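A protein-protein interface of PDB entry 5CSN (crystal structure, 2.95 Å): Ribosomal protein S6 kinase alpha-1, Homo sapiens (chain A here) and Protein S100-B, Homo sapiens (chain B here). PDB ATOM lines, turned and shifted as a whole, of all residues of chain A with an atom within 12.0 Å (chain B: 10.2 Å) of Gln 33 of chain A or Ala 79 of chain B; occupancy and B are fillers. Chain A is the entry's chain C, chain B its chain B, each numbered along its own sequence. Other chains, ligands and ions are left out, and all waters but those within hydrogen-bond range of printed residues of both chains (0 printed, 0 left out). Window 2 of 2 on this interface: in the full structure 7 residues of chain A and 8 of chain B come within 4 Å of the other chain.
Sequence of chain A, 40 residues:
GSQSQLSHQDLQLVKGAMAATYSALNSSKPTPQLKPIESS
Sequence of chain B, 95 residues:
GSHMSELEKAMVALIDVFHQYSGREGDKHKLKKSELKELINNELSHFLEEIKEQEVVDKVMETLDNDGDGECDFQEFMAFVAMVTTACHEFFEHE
Of the printed residues of chain B, Leu 25 of chain A touches Thr 63 (3.6 Å).
Printed residues of chain B within 4 Å of Ser 27 of chain A: Met 83.
Gln 33 of chain A touches two residues of chain B.
No residue of chain B comes within 4 Å of Leu 34 of chain A.
Of the printed residues of chain B, Lys 35 of chain A touches Gln 75 (3.6 Å).
Of the printed residues of chain A, Thr 63 of chain B touches Leu 25 (3.6 Å).
No residue of chain A comes within 4 Å of Leu 64 of chain B.
Of the printed residues of chain A, Gln 75 of chain B touches Lys 35.
No residue of chain A comes within 4 Å of Phe 77 of chain B.
No residue of chain A comes within 4 Å of Met 78 of chain B.
Ala 79 of chain B touches just one residue of chain A: Gln 33.
No residue of chain A comes within 4 Å of Phe 80 of chain B.
No residue of chain A comes within 4 Å of Val 81 of chain B.
Met 83 of chain B touches just one residue of chain A: Ser 27.
The nearest residue of chain B that does not touch Gln 33 of chain A is Met 78 of chain B (5.0 Å).
Hydrophobic or aromatic side chains of chain B that line the printed part of chain A: Ala 79, Ala 82 and Met 83.
Of the 13 printed residues of chain A, 4 touch a printed residue of chain B.
Hydrophobic or aromatic side chains of chain A that line the printed part of chain B: Leu 25.
Among the printed residues, 5 pairs touch across the chains.
Among the printed residues, no Asp or Glu carboxylate lies within 4 Å of a Lys or Arg side-chain nitrogen of the other chain.
The side-chain hydroxyl (OG) of Ser 27 of chain A sits at hydrogen-bond distance from the backbone carbonyl oxygen (O) of Ala 24 of chain A, 3.5 Å away.
The side-chain hydroxyl (OG1) of Thr 86 of chain B lies within hydrogen-bond range of the backbone carbonyl oxygen (O) of Ala 82 of chain B, at 2.9 Å.
The side-chain hydroxyl (OG) of Ser 28 of chain A is in hydrogen-bond range of the backbone carbonyl oxygen (O) of Leu 25 of chain A (2.9 Å).
The backbone NH of Gln 75 of chain B sits close to the side-chain carboxylate of Asp 73 of chain B (3.4 Å).
Thr 63 of chain B touches Leu 25 of chain A.
Ser 27 of chain A touches Met 83 of chain B.
NE2 of Gln 33 of chain A touches CB of Ala 79 of chain B, at 3.9 Å.
Ala 82 of chain B touches Gln 33 of chain A.
Lys 35 of chain A touches Gln 75 of chain B (CD to NE2, 3.6 Å).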
ATOM      1  N   SER A  23      -6.309  -6.412 -24.521  1.00  0.00           N
ATOM      2  CA  SER A  23      -6.261  -6.110 -23.097  1.00  0.00           C
ATOM      3  C   SER A  23      -5.522  -7.172 -22.292  1.00  0.00           C
ATOM      4  O   SER A  23      -4.993  -6.899 -21.210  1.00  0.00           O
ATOM      5  CB  SER A  23      -7.679  -5.954 -22.537  1.00  0.00           C
ATOM      6  OG  SER A  23      -8.418  -4.988 -23.267  1.00  0.00           O
ATOM      7  N   ALA A  24      -5.528  -8.395 -22.810  1.00  0.00           N
ATOM      8  CA  ALA A  24      -4.853  -9.505 -22.151  1.00  0.00           C
ATOM      9  C   ALA A  24      -3.350  -9.280 -22.200  1.00  0.00           C
ATOM     10  O   ALA A  24      -2.675  -9.376 -21.172  1.00  0.00           O
ATOM     11  CB  ALA A  24      -5.238 -10.831 -22.782  1.00  0.00           C
ATOM     12  N   LEU A  25      -2.824  -8.966 -23.381  1.00  0.00           N
ATOM     13  CA  LEU A  25      -1.403  -8.660 -23.525  1.00  0.00           C
ATOM     14  C   LEU A  25      -1.037  -7.390 -22.769  1.00  0.00           C
ATOM     15  O   LEU A  25       0.118  -7.209 -22.370  1.00  0.00           O
ATOM     16  CB  LEU A  25      -1.025  -8.504 -25.005  1.00  0.00           C
ATOM     17  CG  LEU A  25      -0.749  -9.765 -25.827  1.00  0.00           C
ATOM     18  CD1 LEU A  25      -0.820  -9.446 -27.311  1.00  0.00           C
ATOM     19  CD2 LEU A  25       0.611 -10.348 -25.471  1.00  0.00           C
ATOM     20  N   ASN A  26      -2.028  -6.522 -22.574  1.00  0.00           N
ATOM     21  CA  ASN A  26      -1.834  -5.246 -21.889  1.00  0.00           C
ATOM     22  C   ASN A  26      -1.531  -5.385 -20.400  1.00  0.00           C
ATOM     23  O   ASN A  26      -1.062  -4.441 -19.771  1.00  0.00           O
ATOM     24  CB  ASN A  26      -3.076  -4.362 -22.074  1.00  0.00           C
ATOM     25  CG  ASN A  26      -2.779  -3.074 -22.821  1.00  0.00           C
ATOM     26  OD1 ASN A  26      -2.794  -3.043 -24.051  1.00  0.00           O
ATOM     27  ND2 ASN A  26      -2.505  -2.006 -22.080  1.00  0.00           N
ATOM     28  N   SER A  27      -1.801  -6.559 -19.840  1.00  0.00           N
ATOM     29  CA  SER A  27      -1.538  -6.795 -18.424  1.00  0.00           C
ATOM     30  C   SER A  27      -0.655  -8.025 -18.213  1.00  0.00           C
ATOM     31  O   SER A  27      -0.811  -8.757 -17.236  1.00  0.00           O
ATOM     32  CB  SER A  27      -2.851  -6.946 -17.647  1.00  0.00           C
ATOM     33  OG  SER A  27      -3.616  -8.035 -18.131  1.00  0.00           O
ATOM     34  N   SER A  28       0.270  -8.248 -19.141  1.00  0.00           N
ATOM     35  CA  SER A  28       1.260  -9.309 -19.000  1.00  0.00           C
ATOM     36  C   SER A  28       2.587  -8.716 -18.539  1.00  0.00           C
ATOM     37  O   SER A  28       3.375  -9.374 -17.858  1.00  0.00           O
ATOM     38  CB  SER A  28       1.440 -10.068 -20.316  1.00  0.00           C
ATOM     39  OG  SER A  28       1.886  -9.206 -21.349  1.00  0.00           O
ATOM     40  N   LYS A  29       2.817  -7.463 -18.918  1.00  0.00           N
ATOM     41  CA  LYS A  29       4.024  -6.722 -18.547  1.00  0.00           C
ATOM     42  C   LYS A  29       3.886  -5.865 -17.278  1.00  0.00           C
ATOM     43  O   LYS A  29       4.840  -5.785 -16.500  1.00  0.00           O
ATOM     44  CB  LYS A  29       4.474  -5.840 -19.715  1.00  0.00           C
ATOM     45  CG  LYS A  29       5.448  -4.731 -19.356  1.00  0.00           C
ATOM     46  CD  LYS A  29       4.834  -3.372 -19.648  1.00  0.00           C
ATOM     47  CE  LYS A  29       5.861  -2.260 -19.543  1.00  0.00           C
ATOM     48  NZ  LYS A  29       5.286  -0.950 -19.954  1.00  0.00           N
ATOM     49  N   PRO A  30       2.718  -5.210 -17.063  1.00  0.00           N
ATOM     50  CA  PRO A  30       2.524  -4.511 -15.784  1.00  0.00           C
ATOM     51  C   PRO A  30       2.853  -5.370 -14.565  1.00  0.00           C
ATOM     52  O   PRO A  30       3.205  -4.837 -13.512  1.00  0.00           O
ATOM     53  CB  PRO A  30       1.040  -4.155 -15.810  1.00  0.00           C
ATOM     54  CG  PRO A  30       0.768  -3.912 -17.239  1.00  0.00           C
ATOM     55  CD  PRO A  30       1.622  -4.898 -18.002  1.00  0.00           C
ATOM     56  N   THR A  31       2.736  -6.684 -14.716  1.00  0.00           N
ATOM     57  CA  THR A  31       3.211  -7.613 -13.703  1.00  0.00           C
ATOM     58  C   THR A  31       3.520  -8.982 -14.278  1.00  0.00           C
ATOM     59  O   THR A  31       2.646  -9.633 -14.850  1.00  0.00           O
ATOM     60  CB  THR A  31       2.188  -7.803 -12.571  1.00  0.00           C
ATOM     61  OG1 THR A  31       0.994  -7.078 -12.879  1.00  0.00           O
ATOM     62  CG2 THR A  31       2.760  -7.324 -11.242  1.00  0.00           C
ATOM     63  N   PRO A  32       4.774  -9.426 -14.128  1.00  0.00           N
ATOM     64  CA  PRO A  32       5.017 -10.866 -14.180  1.00  0.00           C
ATOM     65  C   PRO A  32       4.512 -11.471 -12.875  1.00  0.00           C
ATOM     66  O   PRO A  32       3.465 -11.054 -12.378  1.00  0.00           O
ATOM     67  CB  PRO A  32       6.537 -10.969 -14.313  1.00  0.00           C
ATOM     68  CG  PRO A  32       7.048  -9.713 -13.689  1.00  0.00           C
ATOM     69  CD  PRO A  32       6.021  -8.653 -13.988  1.00  0.00           C
ATOM     70  N   GLN A  33       5.236 -12.425 -12.307  1.00  0.00           N
ATOM     71  CA  GLN A  33       4.842 -12.945 -11.005  1.00  0.00           C
ATOM     72  C   GLN A  33       6.049 -13.219 -10.122  1.00  0.00           C
ATOM     73  O   GLN A  33       6.961 -13.948 -10.511  1.00  0.00           O
ATOM     74  CB  GLN A  33       4.008 -14.226 -11.156  1.00  0.00           C
ATOM     75  CG  GLN A  33       2.692 -14.039 -11.904  1.00  0.00           C
ATOM     76  CD  GLN A  33       1.541 -14.802 -11.283  1.00  0.00           C
ATOM     77  OE1 GLN A  33       0.571 -14.209 -10.812  1.00  0.00           O
ATOM     78  NE2 GLN A  33       1.636 -16.127 -11.286  1.00  0.00           N
ATOM     79  N   LEU A  34       6.054 -12.625  -8.932  1.00  0.00           N
ATOM     80  CA  LEU A  34       6.993 -13.032  -7.897  1.00  0.00           C
ATOM     81  C   LEU A  34       6.478 -14.339  -7.307  1.00  0.00           C
ATOM     82  O   LEU A  34       6.102 -14.401  -6.136  1.00  0.00           O
ATOM     83  CB  LEU A  34       7.137 -11.966  -6.809  1.00  0.00           C
ATOM     84  CG  LEU A  34       7.529 -10.539  -7.199  1.00  0.00           C
ATOM     85  CD1 LEU A  34       8.035  -9.791  -5.974  1.00  0.00           C
ATOM     86  CD2 LEU A  34       8.567 -10.524  -8.312  1.00  0.00           C
ATOM     87  N   LYS A  35       6.455 -15.376  -8.141  1.00  0.00           N
ATOM     88  CA  LYS A  35       5.817 -16.644  -7.814  1.00  0.00           C
ATOM     89  C   LYS A  35       6.375 -17.268  -6.541  1.00  0.00           C
ATOM     90  O   LYS A  35       5.725 -17.241  -5.496  1.00  0.00           O
ATOM     91  CB  LYS A  35       5.967 -17.622  -8.981  1.00  0.00           C
ATOM     92  CG  LYS A  35       7.405 -17.848  -9.411  1.00  0.00           C
ATOM     93  CD  LYS A  35       7.683 -19.326  -9.602  1.00  0.00           C
ATOM     94  CE  LYS A  35       7.388 -20.101  -8.326  1.00  0.00           C
ATOM     95  NZ  LYS A  35       7.655 -21.556  -8.478  1.00  0.00           N
ATOM     96  N   LEU B  14     -11.019 -23.051  -9.399  1.00  0.00           N
ATOM     97  CA  LEU B  14      -9.968 -22.843 -10.389  1.00  0.00           C
ATOM     98  C   LEU B  14      -9.289 -24.176 -10.686  1.00  0.00           C
ATOM     99  O   LEU B  14      -9.006 -24.500 -11.839  1.00  0.00           O
ATOM    100  CB  LEU B  14      -8.947 -21.818  -9.895  1.00  0.00           C
ATOM    101  CG  LEU B  14      -9.511 -20.449  -9.508  1.00  0.00           C
ATOM    102  CD1 LEU B  14      -8.392 -19.469  -9.209  1.00  0.00           C
ATOM    103  CD2 LEU B  14     -10.428 -19.908 -10.592  1.00  0.00           C
ATOM    104  N   PHE B  18      -9.676 -26.484 -14.333  1.00  0.00           N
ATOM    105  CA  PHE B  18      -8.450 -26.855 -15.024  1.00  0.00           C
ATOM    106  C   PHE B  18      -8.478 -28.346 -15.323  1.00  0.00           C
ATOM    107  O   PHE B  18      -8.261 -28.766 -16.457  1.00  0.00           O
ATOM    108  CB  PHE B  18      -7.219 -26.499 -14.186  1.00  0.00           C
ATOM    109  CG  PHE B  18      -5.914 -26.900 -14.820  1.00  0.00           C
ATOM    110  CD1 PHE B  18      -5.360 -26.137 -15.837  1.00  0.00           C
ATOM    111  CD2 PHE B  18      -5.242 -28.037 -14.401  1.00  0.00           C
ATOM    112  CE1 PHE B  18      -4.159 -26.500 -16.422  1.00  0.00           C
ATOM    113  CE2 PHE B  18      -4.041 -28.405 -14.983  1.00  0.00           C
ATOM    114  CZ  PHE B  18      -3.500 -27.635 -15.995  1.00  0.00           C
ATOM    115  N   LEU B  44     -15.217 -18.967 -20.283  1.00  0.00           N
ATOM    116  CA  LEU B  44     -14.922 -17.533 -20.237  1.00  0.00           C
ATOM    117  C   LEU B  44     -15.646 -16.736 -21.325  1.00  0.00           C
ATOM    118  O   LEU B  44     -15.132 -15.728 -21.810  1.00  0.00           O
ATOM    119  CB  LEU B  44     -13.413 -17.300 -20.333  1.00  0.00           C
ATOM    120  CG  LEU B  44     -12.591 -17.810 -19.145  1.00  0.00           C
ATOM    121  CD1 LEU B  44     -11.103 -17.663 -19.413  1.00  0.00           C
ATOM    122  CD2 LEU B  44     -12.980 -17.073 -17.870  1.00  0.00           C
ATOM    123  N   VAL B  60      -2.366 -16.990 -27.825  1.00  0.00           N
ATOM    124  CA  VAL B  60      -2.723 -17.117 -26.414  1.00  0.00           C
ATOM    125  C   VAL B  60      -1.826 -18.123 -25.701  1.00  0.00           C
ATOM    126  O   VAL B  60      -1.314 -17.848 -24.615  1.00  0.00           O
ATOM    127  CB  VAL B  60      -4.196 -17.541 -26.241  1.00  0.00           C
ATOM    128  CG1 VAL B  60      -4.516 -17.773 -24.773  1.00  0.00           C
ATOM    129  CG2 VAL B  60      -5.123 -16.491 -26.835  1.00  0.00           C
ATOM    130  N   THR B  63       1.690 -16.729 -25.184  1.00  0.00           N
ATOM    131  CA  THR B  63       1.813 -15.809 -24.065  1.00  0.00           C
ATOM    132  C   THR B  63       1.708 -16.576 -22.754  1.00  0.00           C
ATOM    133  O   THR B  63       2.363 -16.235 -21.768  1.00  0.00           O
ATOM    134  CB  THR B  63       0.726 -14.709 -24.114  1.00  0.00           C
ATOM    135  OG1 THR B  63       0.849 -13.964 -25.331  1.00  0.00           O
ATOM    136  CG2 THR B  63       0.855 -13.759 -22.929  1.00  0.00           C
ATOM    137  N   LEU B  64       0.890 -17.624 -22.750  1.00  0.00           N
ATOM    138  CA  LEU B  64       0.675 -18.397 -21.534  1.00  0.00           C
ATOM    139  C   LEU B  64       1.807 -19.371 -21.211  1.00  0.00           C
ATOM    140  O   LEU B  64       2.087 -19.645 -20.045  1.00  0.00           O
ATOM    141  CB  LEU B  64      -0.638 -19.166 -21.645  1.00  0.00           C
ATOM    142  CG  LEU B  64      -1.815 -18.448 -20.994  1.00  0.00           C
ATOM    143  CD1 LEU B  64      -2.935 -19.427 -20.675  1.00  0.00           C
ATOM    144  CD2 LEU B  64      -1.332 -17.705 -19.758  1.00  0.00           C
ATOM    145  N   ASP B  65       2.454 -19.887 -22.251  1.00  0.00           N
ATOM    146  CA  ASP B  65       3.460 -20.934 -22.090  1.00  0.00           C
ATOM    147  C   ASP B  65       4.814 -20.328 -21.750  1.00  0.00           C
ATOM    148  O   ASP B  65       5.449 -19.711 -22.605  1.00  0.00           O
ATOM    149  CB  ASP B  65       3.569 -21.798 -23.347  1.00  0.00           C
ATOM    150  CG  ASP B  65       4.346 -23.084 -23.106  1.00  0.00           C
ATOM    151  OD1 ASP B  65       4.425 -23.531 -21.937  1.00  0.00           O
ATOM    152  OD2 ASP B  65       4.879 -23.645 -24.086  1.00  0.00           O
ATOM    153  N   ASN B  66       5.260 -20.489 -20.510  1.00  0.00           N
ATOM    154  CA  ASN B  66       6.506 -19.860 -20.092  1.00  0.00           C
ATOM    155  C   ASN B  66       7.642 -20.874 -19.999  1.00  0.00           C
ATOM    156  O   ASN B  66       8.816 -20.508 -20.045  1.00  0.00           O
ATOM    157  CB  ASN B  66       6.320 -19.157 -18.747  1.00  0.00           C
ATOM    158  CG  ASN B  66       5.373 -17.977 -18.836  1.00  0.00           C
ATOM    159  OD1 ASN B  66       5.306 -17.294 -19.857  1.00  0.00           O
ATOM    160  ND2 ASN B  66       4.628 -17.736 -17.763  1.00  0.00           N
ATOM    161  N   ASP B  67       7.285 -22.147 -19.871  1.00  0.00           N
ATOM    162  CA  ASP B  67       8.276 -23.217 -19.803  1.00  0.00           C
ATOM    163  C   ASP B  67       8.564 -23.838 -21.172  1.00  0.00           C
ATOM    164  O   ASP B  67       9.436 -24.697 -21.292  1.00  0.00           O
ATOM    165  CB  ASP B  67       7.825 -24.300 -18.822  1.00  0.00           C
ATOM    166  CG  ASP B  67       6.529 -24.957 -19.239  1.00  0.00           C
ATOM    167  OD1 ASP B  67       5.835 -24.393 -20.109  1.00  0.00           O
ATOM    168  OD2 ASP B  67       6.206 -26.038 -18.700  1.00  0.00           O
ATOM    169  N   CYS B  72      -0.316 -25.815 -21.451  1.00  0.00           N
ATOM    170  CA  CYS B  72      -0.513 -24.967 -20.288  1.00  0.00           C
ATOM    171  C   CYS B  72      -0.671 -25.812 -19.023  1.00  0.00           C
ATOM    172  O   CYS B  72      -1.680 -26.498 -18.865  1.00  0.00           O
ATOM    173  CB  CYS B  72      -1.729 -24.060 -20.483  1.00  0.00           C
ATOM    174  SG  CYS B  72      -2.092 -23.006 -19.065  1.00  0.00           S
ATOM    175  N   ASP B  73       0.316 -25.786 -18.133  1.00  0.00           N
ATOM    176  CA  ASP B  73       0.178 -26.504 -16.870  1.00  0.00           C
ATOM    177  C   ASP B  73      -0.586 -25.617 -15.888  1.00  0.00           C
ATOM    178  O   ASP B  73      -0.988 -24.509 -16.244  1.00  0.00           O
ATOM    179  CB  ASP B  73       1.545 -26.934 -16.311  1.00  0.00           C
ATOM    180  CG  ASP B  73       2.384 -25.770 -15.801  1.00  0.00           C
ATOM    181  OD1 ASP B  73       2.011 -24.599 -16.007  1.00  0.00           O
ATOM    182  OD2 ASP B  73       3.437 -26.035 -15.184  1.00  0.00           O
ATOM    183  N   PHE B  74      -0.791 -26.092 -14.663  1.00  0.00           N
ATOM    184  CA  PHE B  74      -1.638 -25.365 -13.722  1.00  0.00           C
ATOM    185  C   PHE B  74      -1.017 -24.030 -13.323  1.00  0.00           C
ATOM    186  O   PHE B  74      -1.716 -23.024 -13.207  1.00  0.00           O
ATOM    187  CB  PHE B  74      -1.906 -26.196 -12.469  1.00  0.00           C
ATOM    188  CG  PHE B  74      -2.874 -25.551 -11.521  1.00  0.00           C
ATOM    189  CD1 PHE B  74      -4.227 -25.506 -11.817  1.00  0.00           C
ATOM    190  CD2 PHE B  74      -2.432 -24.968 -10.344  1.00  0.00           C
ATOM    191  CE1 PHE B  74      -5.122 -24.908 -10.950  1.00  0.00           C
ATOM    192  CE2 PHE B  74      -3.322 -24.368  -9.474  1.00  0.00           C
ATOM    193  CZ  PHE B  74      -4.669 -24.337  -9.779  1.00  0.00           C
ATOM    194  N   GLN B  75       0.295 -24.032 -13.106  1.00  0.00           N
ATOM    195  CA  GLN B  75       1.015 -22.826 -12.709  1.00  0.00           C
ATOM    196  C   GLN B  75       0.860 -21.723 -13.757  1.00  0.00           C
ATOM    197  O   GLN B  75       0.609 -20.566 -13.425  1.00  0.00           O
ATOM    198  CB  GLN B  75       2.494 -23.137 -12.466  1.00  0.00           C
ATOM    199  CG  GLN B  75       3.293 -21.966 -11.918  1.00  0.00           C
ATOM    200  CD  GLN B  75       4.665 -22.374 -11.421  1.00  0.00           C
ATOM    201  OE1 GLN B  75       4.837 -23.450 -10.847  1.00  0.00           O
ATOM    202  NE2 GLN B  75       5.658 -21.531 -11.673  1.00  0.00           N
ATOM    203  N   GLU B  76       1.010 -22.098 -15.023  1.00  0.00           N
ATOM    204  CA  GLU B  76       0.864 -21.168 -16.135  1.00  0.00           C
ATOM    205  C   GLU B  76      -0.581 -20.696 -16.267  1.00  0.00           C
ATOM    206  O   GLU B  76      -0.845 -19.552 -16.638  1.00  0.00           O
ATOM    207  CB  GLU B  76       1.306 -21.831 -17.446  1.00  0.00           C
ATOM    208  CG  GLU B  76       2.810 -22.024 -17.616  1.00  0.00           C
ATOM    209  CD  GLU B  76       3.134 -23.099 -18.645  1.00  0.00           C
ATOM    210  OE1 GLU B  76       2.306 -24.018 -18.825  1.00  0.00           O
ATOM    211  OE2 GLU B  76       4.208 -23.034 -19.279  1.00  0.00           O
ATOM    212  N   PHE B  77      -1.510 -21.597 -15.962  1.00  0.00           N
ATOM    213  CA  PHE B  77      -2.938 -21.293 -15.960  1.00  0.00           C
ATOM    214  C   PHE B  77      -3.360 -20.302 -14.871  1.00  0.00           C
ATOM    215  O   PHE B  77      -4.231 -19.462 -15.096  1.00  0.00           O
ATOM    216  CB  PHE B  77      -3.737 -22.593 -15.819  1.00  0.00           C
ATOM    217  CG  PHE B  77      -5.206 -22.387 -15.596  1.00  0.00           C
ATOM    218  CD1 PHE B  77      -6.023 -21.977 -16.637  1.00  0.00           C
ATOM    219  CD2 PHE B  77      -5.776 -22.622 -14.355  1.00  0.00           C
ATOM    220  CE1 PHE B  77      -7.380 -21.791 -16.444  1.00  0.00           C
ATOM    221  CE2 PHE B  77      -7.133 -22.440 -14.155  1.00  0.00           C
ATOM    222  CZ  PHE B  77      -7.936 -22.024 -15.200  1.00  0.00           C
ATOM    223  N   MET B  78      -2.761 -20.405 -13.689  1.00  0.00           N
ATOM    224  CA  MET B  78      -3.059 -19.466 -12.609  1.00  0.00           C
ATOM    225  C   MET B  78      -2.640 -18.048 -12.974  1.00  0.00           C
ATOM    226  O   MET B  78      -3.318 -17.081 -12.624  1.00  0.00           O
ATOM    227  CB  MET B  78      -2.381 -19.897 -11.310  1.00  0.00           C
ATOM    228  CG  MET B  78      -3.086 -21.038 -10.606  1.00  0.00           C
ATOM    229  SD  MET B  78      -4.842 -20.706 -10.348  1.00  0.00           S
ATOM    230  CE  MET B  78      -4.782 -19.197  -9.392  1.00  0.00           C
ATOM    231  N   ALA B  79      -1.513 -17.936 -13.668  1.00  0.00           N
ATOM    232  CA  ALA B  79      -1.054 -16.654 -14.185  1.00  0.00           C
ATOM    233  C   ALA B  79      -2.106 -16.071 -15.118  1.00  0.00           C
ATOM    234  O   ALA B  79      -2.418 -14.884 -15.054  1.00  0.00           O
ATOM    235  CB  ALA B  79       0.275 -16.811 -14.903  1.00  0.00           C
ATOM    236  N   PHE B  80      -2.651 -16.925 -15.979  1.00  0.00           N
ATOM    237  CA  PHE B  80      -3.710 -16.539 -16.906  1.00  0.00           C
ATOM    238  C   PHE B  80      -4.941 -16.014 -16.176  1.00  0.00           C
ATOM    239  O   PHE B  80      -5.477 -14.963 -16.526  1.00  0.00           O
ATOM    240  CB  PHE B  80      -4.098 -17.733 -17.775  1.00  0.00           C
ATOM    241  CG  PHE B  80      -5.275 -17.483 -18.666  1.00  0.00           C
ATOM    242  CD1 PHE B  80      -5.206 -16.532 -19.669  1.00  0.00           C
ATOM    243  CD2 PHE B  80      -6.441 -18.213 -18.520  1.00  0.00           C
ATOM    244  CE1 PHE B  80      -6.284 -16.303 -20.500  1.00  0.00           C
ATOM    245  CE2 PHE B  80      -7.522 -17.989 -19.349  1.00  0.00           C
ATOM    246  CZ  PHE B  80      -7.443 -17.034 -20.340  1.00  0.00           C
ATOM    247  N   VAL B  81      -5.393 -16.766 -15.177  1.00  0.00           N
ATOM    248  CA  VAL B  81      -6.510 -16.348 -14.334  1.00  0.00           C
ATOM    249  C   VAL B  81      -6.229 -14.989 -13.696  1.00  0.00           C
ATOM    250  O   VAL B  81      -7.098 -14.120 -13.656  1.00  0.00           O
ATOM    251  CB  VAL B  81      -6.804 -17.391 -13.236  1.00  0.00           C
ATOM    252  CG1 VAL B  81      -7.803 -16.843 -12.230  1.00  0.00           C
ATOM    253  CG2 VAL B  81      -7.326 -18.678 -13.857  1.00  0.00           C
ATOM    254  N   ALA B  82      -5.003 -14.816 -13.209  1.00  0.00           N
ATOM    255  CA  ALA B  82      -4.560 -13.547 -12.640  1.00  0.00           C
ATOM    256  C   ALA B  82      -4.705 -12.404 -13.643  1.00  0.00           C
ATOM    257  O   ALA B  82      -5.167 -11.317 -13.294  1.00  0.00           O
ATOM    258  CB  ALA B  82      -3.124 -13.655 -12.164  1.00  0.00           C
ATOM    259  N   MET B  83      -4.302 -12.656 -14.886  1.00  0.00           N
ATOM    260  CA  MET B  83      -4.301 -11.629 -15.924  1.00  0.00           C
ATOM    261  C   MET B  83      -5.728 -11.197 -16.237  1.00  0.00           C
ATOM    262  O   MET B  83      -6.049 -10.009 -16.236  1.00  0.00           O
ATOM    263  CB  MET B  83      -3.619 -12.136 -17.200  1.00  0.00           C
ATOM    264  CG  MET B  83      -2.148 -12.496 -17.048  1.00  0.00           C
ATOM    265  SD  MET B  83      -1.369 -12.888 -18.630  1.00  0.00           S
ATOM    266  CE  MET B  83       0.172 -13.631 -18.091  1.00  0.00           C
ATOM    267  N   VAL B  84      -6.577 -12.185 -16.503  1.00  0.00           N
ATOM    268  CA  VAL B  84      -7.989 -11.965 -16.803  1.00  0.00           C
ATOM    269  C   VAL B  84      -8.732 -11.281 -15.654  1.00  0.00           C
ATOM    270  O   VAL B  84      -9.487 -10.333 -15.871  1.00  0.00           O
ATOM    271  CB  VAL B  84      -8.693 -13.298 -17.142  1.00  0.00           C
ATOM    272  CG1 VAL B  84     -10.199 -13.107 -17.227  1.00  0.00           C
ATOM    273  CG2 VAL B  84      -8.156 -13.860 -18.448  1.00  0.00           C
ATOM    274  N   THR B  85      -8.499 -11.753 -14.433  1.00  0.00           N
ATOM    275  CA  THR B  85      -9.172 -11.222 -13.250  1.00  0.00           C
ATOM    276  C   THR B  85      -8.829  -9.750 -13.028  1.00  0.00           C
ATOM    277  O   THR B  85      -9.707  -8.940 -12.732  1.00  0.00           O
ATOM    278  CB  THR B  85      -8.810 -12.023 -11.985  1.00  0.00           C
ATOM    279  OG1 THR B  85      -9.029 -13.420 -12.221  1.00  0.00           O
ATOM    280  CG2 THR B  85      -9.659 -11.574 -10.811  1.00  0.00           C
ATOM    281  N   THR B  86      -7.550  -9.417 -13.166  1.00  0.00           N
ATOM    282  CA  THR B  86      -7.074  -8.044 -13.005  1.00  0.00           C
ATOM    283  C   THR B  86      -7.811  -7.097 -13.960  1.00  0.00           C
ATOM    284  O   THR B  86      -8.255  -6.019 -13.566  1.00  0.00           O
ATOM    285  CB  THR B  86      -5.556  -7.951 -13.252  1.00  0.00           C
ATOM    286  OG1 THR B  86      -4.853  -8.629 -12.204  1.00  0.00           O
ATOM    287  CG2 THR B  86      -5.104  -6.501 -13.312  1.00  0.00           C
ATOM    288  N   ALA B  87      -7.938  -7.525 -15.212  1.00  0.00           N
ATOM    289  CA  ALA B  87      -8.621  -6.776 -16.270  1.00  0.00           C
ATOM    290  C   ALA B  87     -10.091  -6.496 -15.944  1.00  0.00           C
ATOM    291  O   ALA B  87     -10.600  -5.402 -16.185  1.00  0.00           O
ATOM    292  CB  ALA B  87      -8.510  -7.523 -17.590  1.00  0.00           C
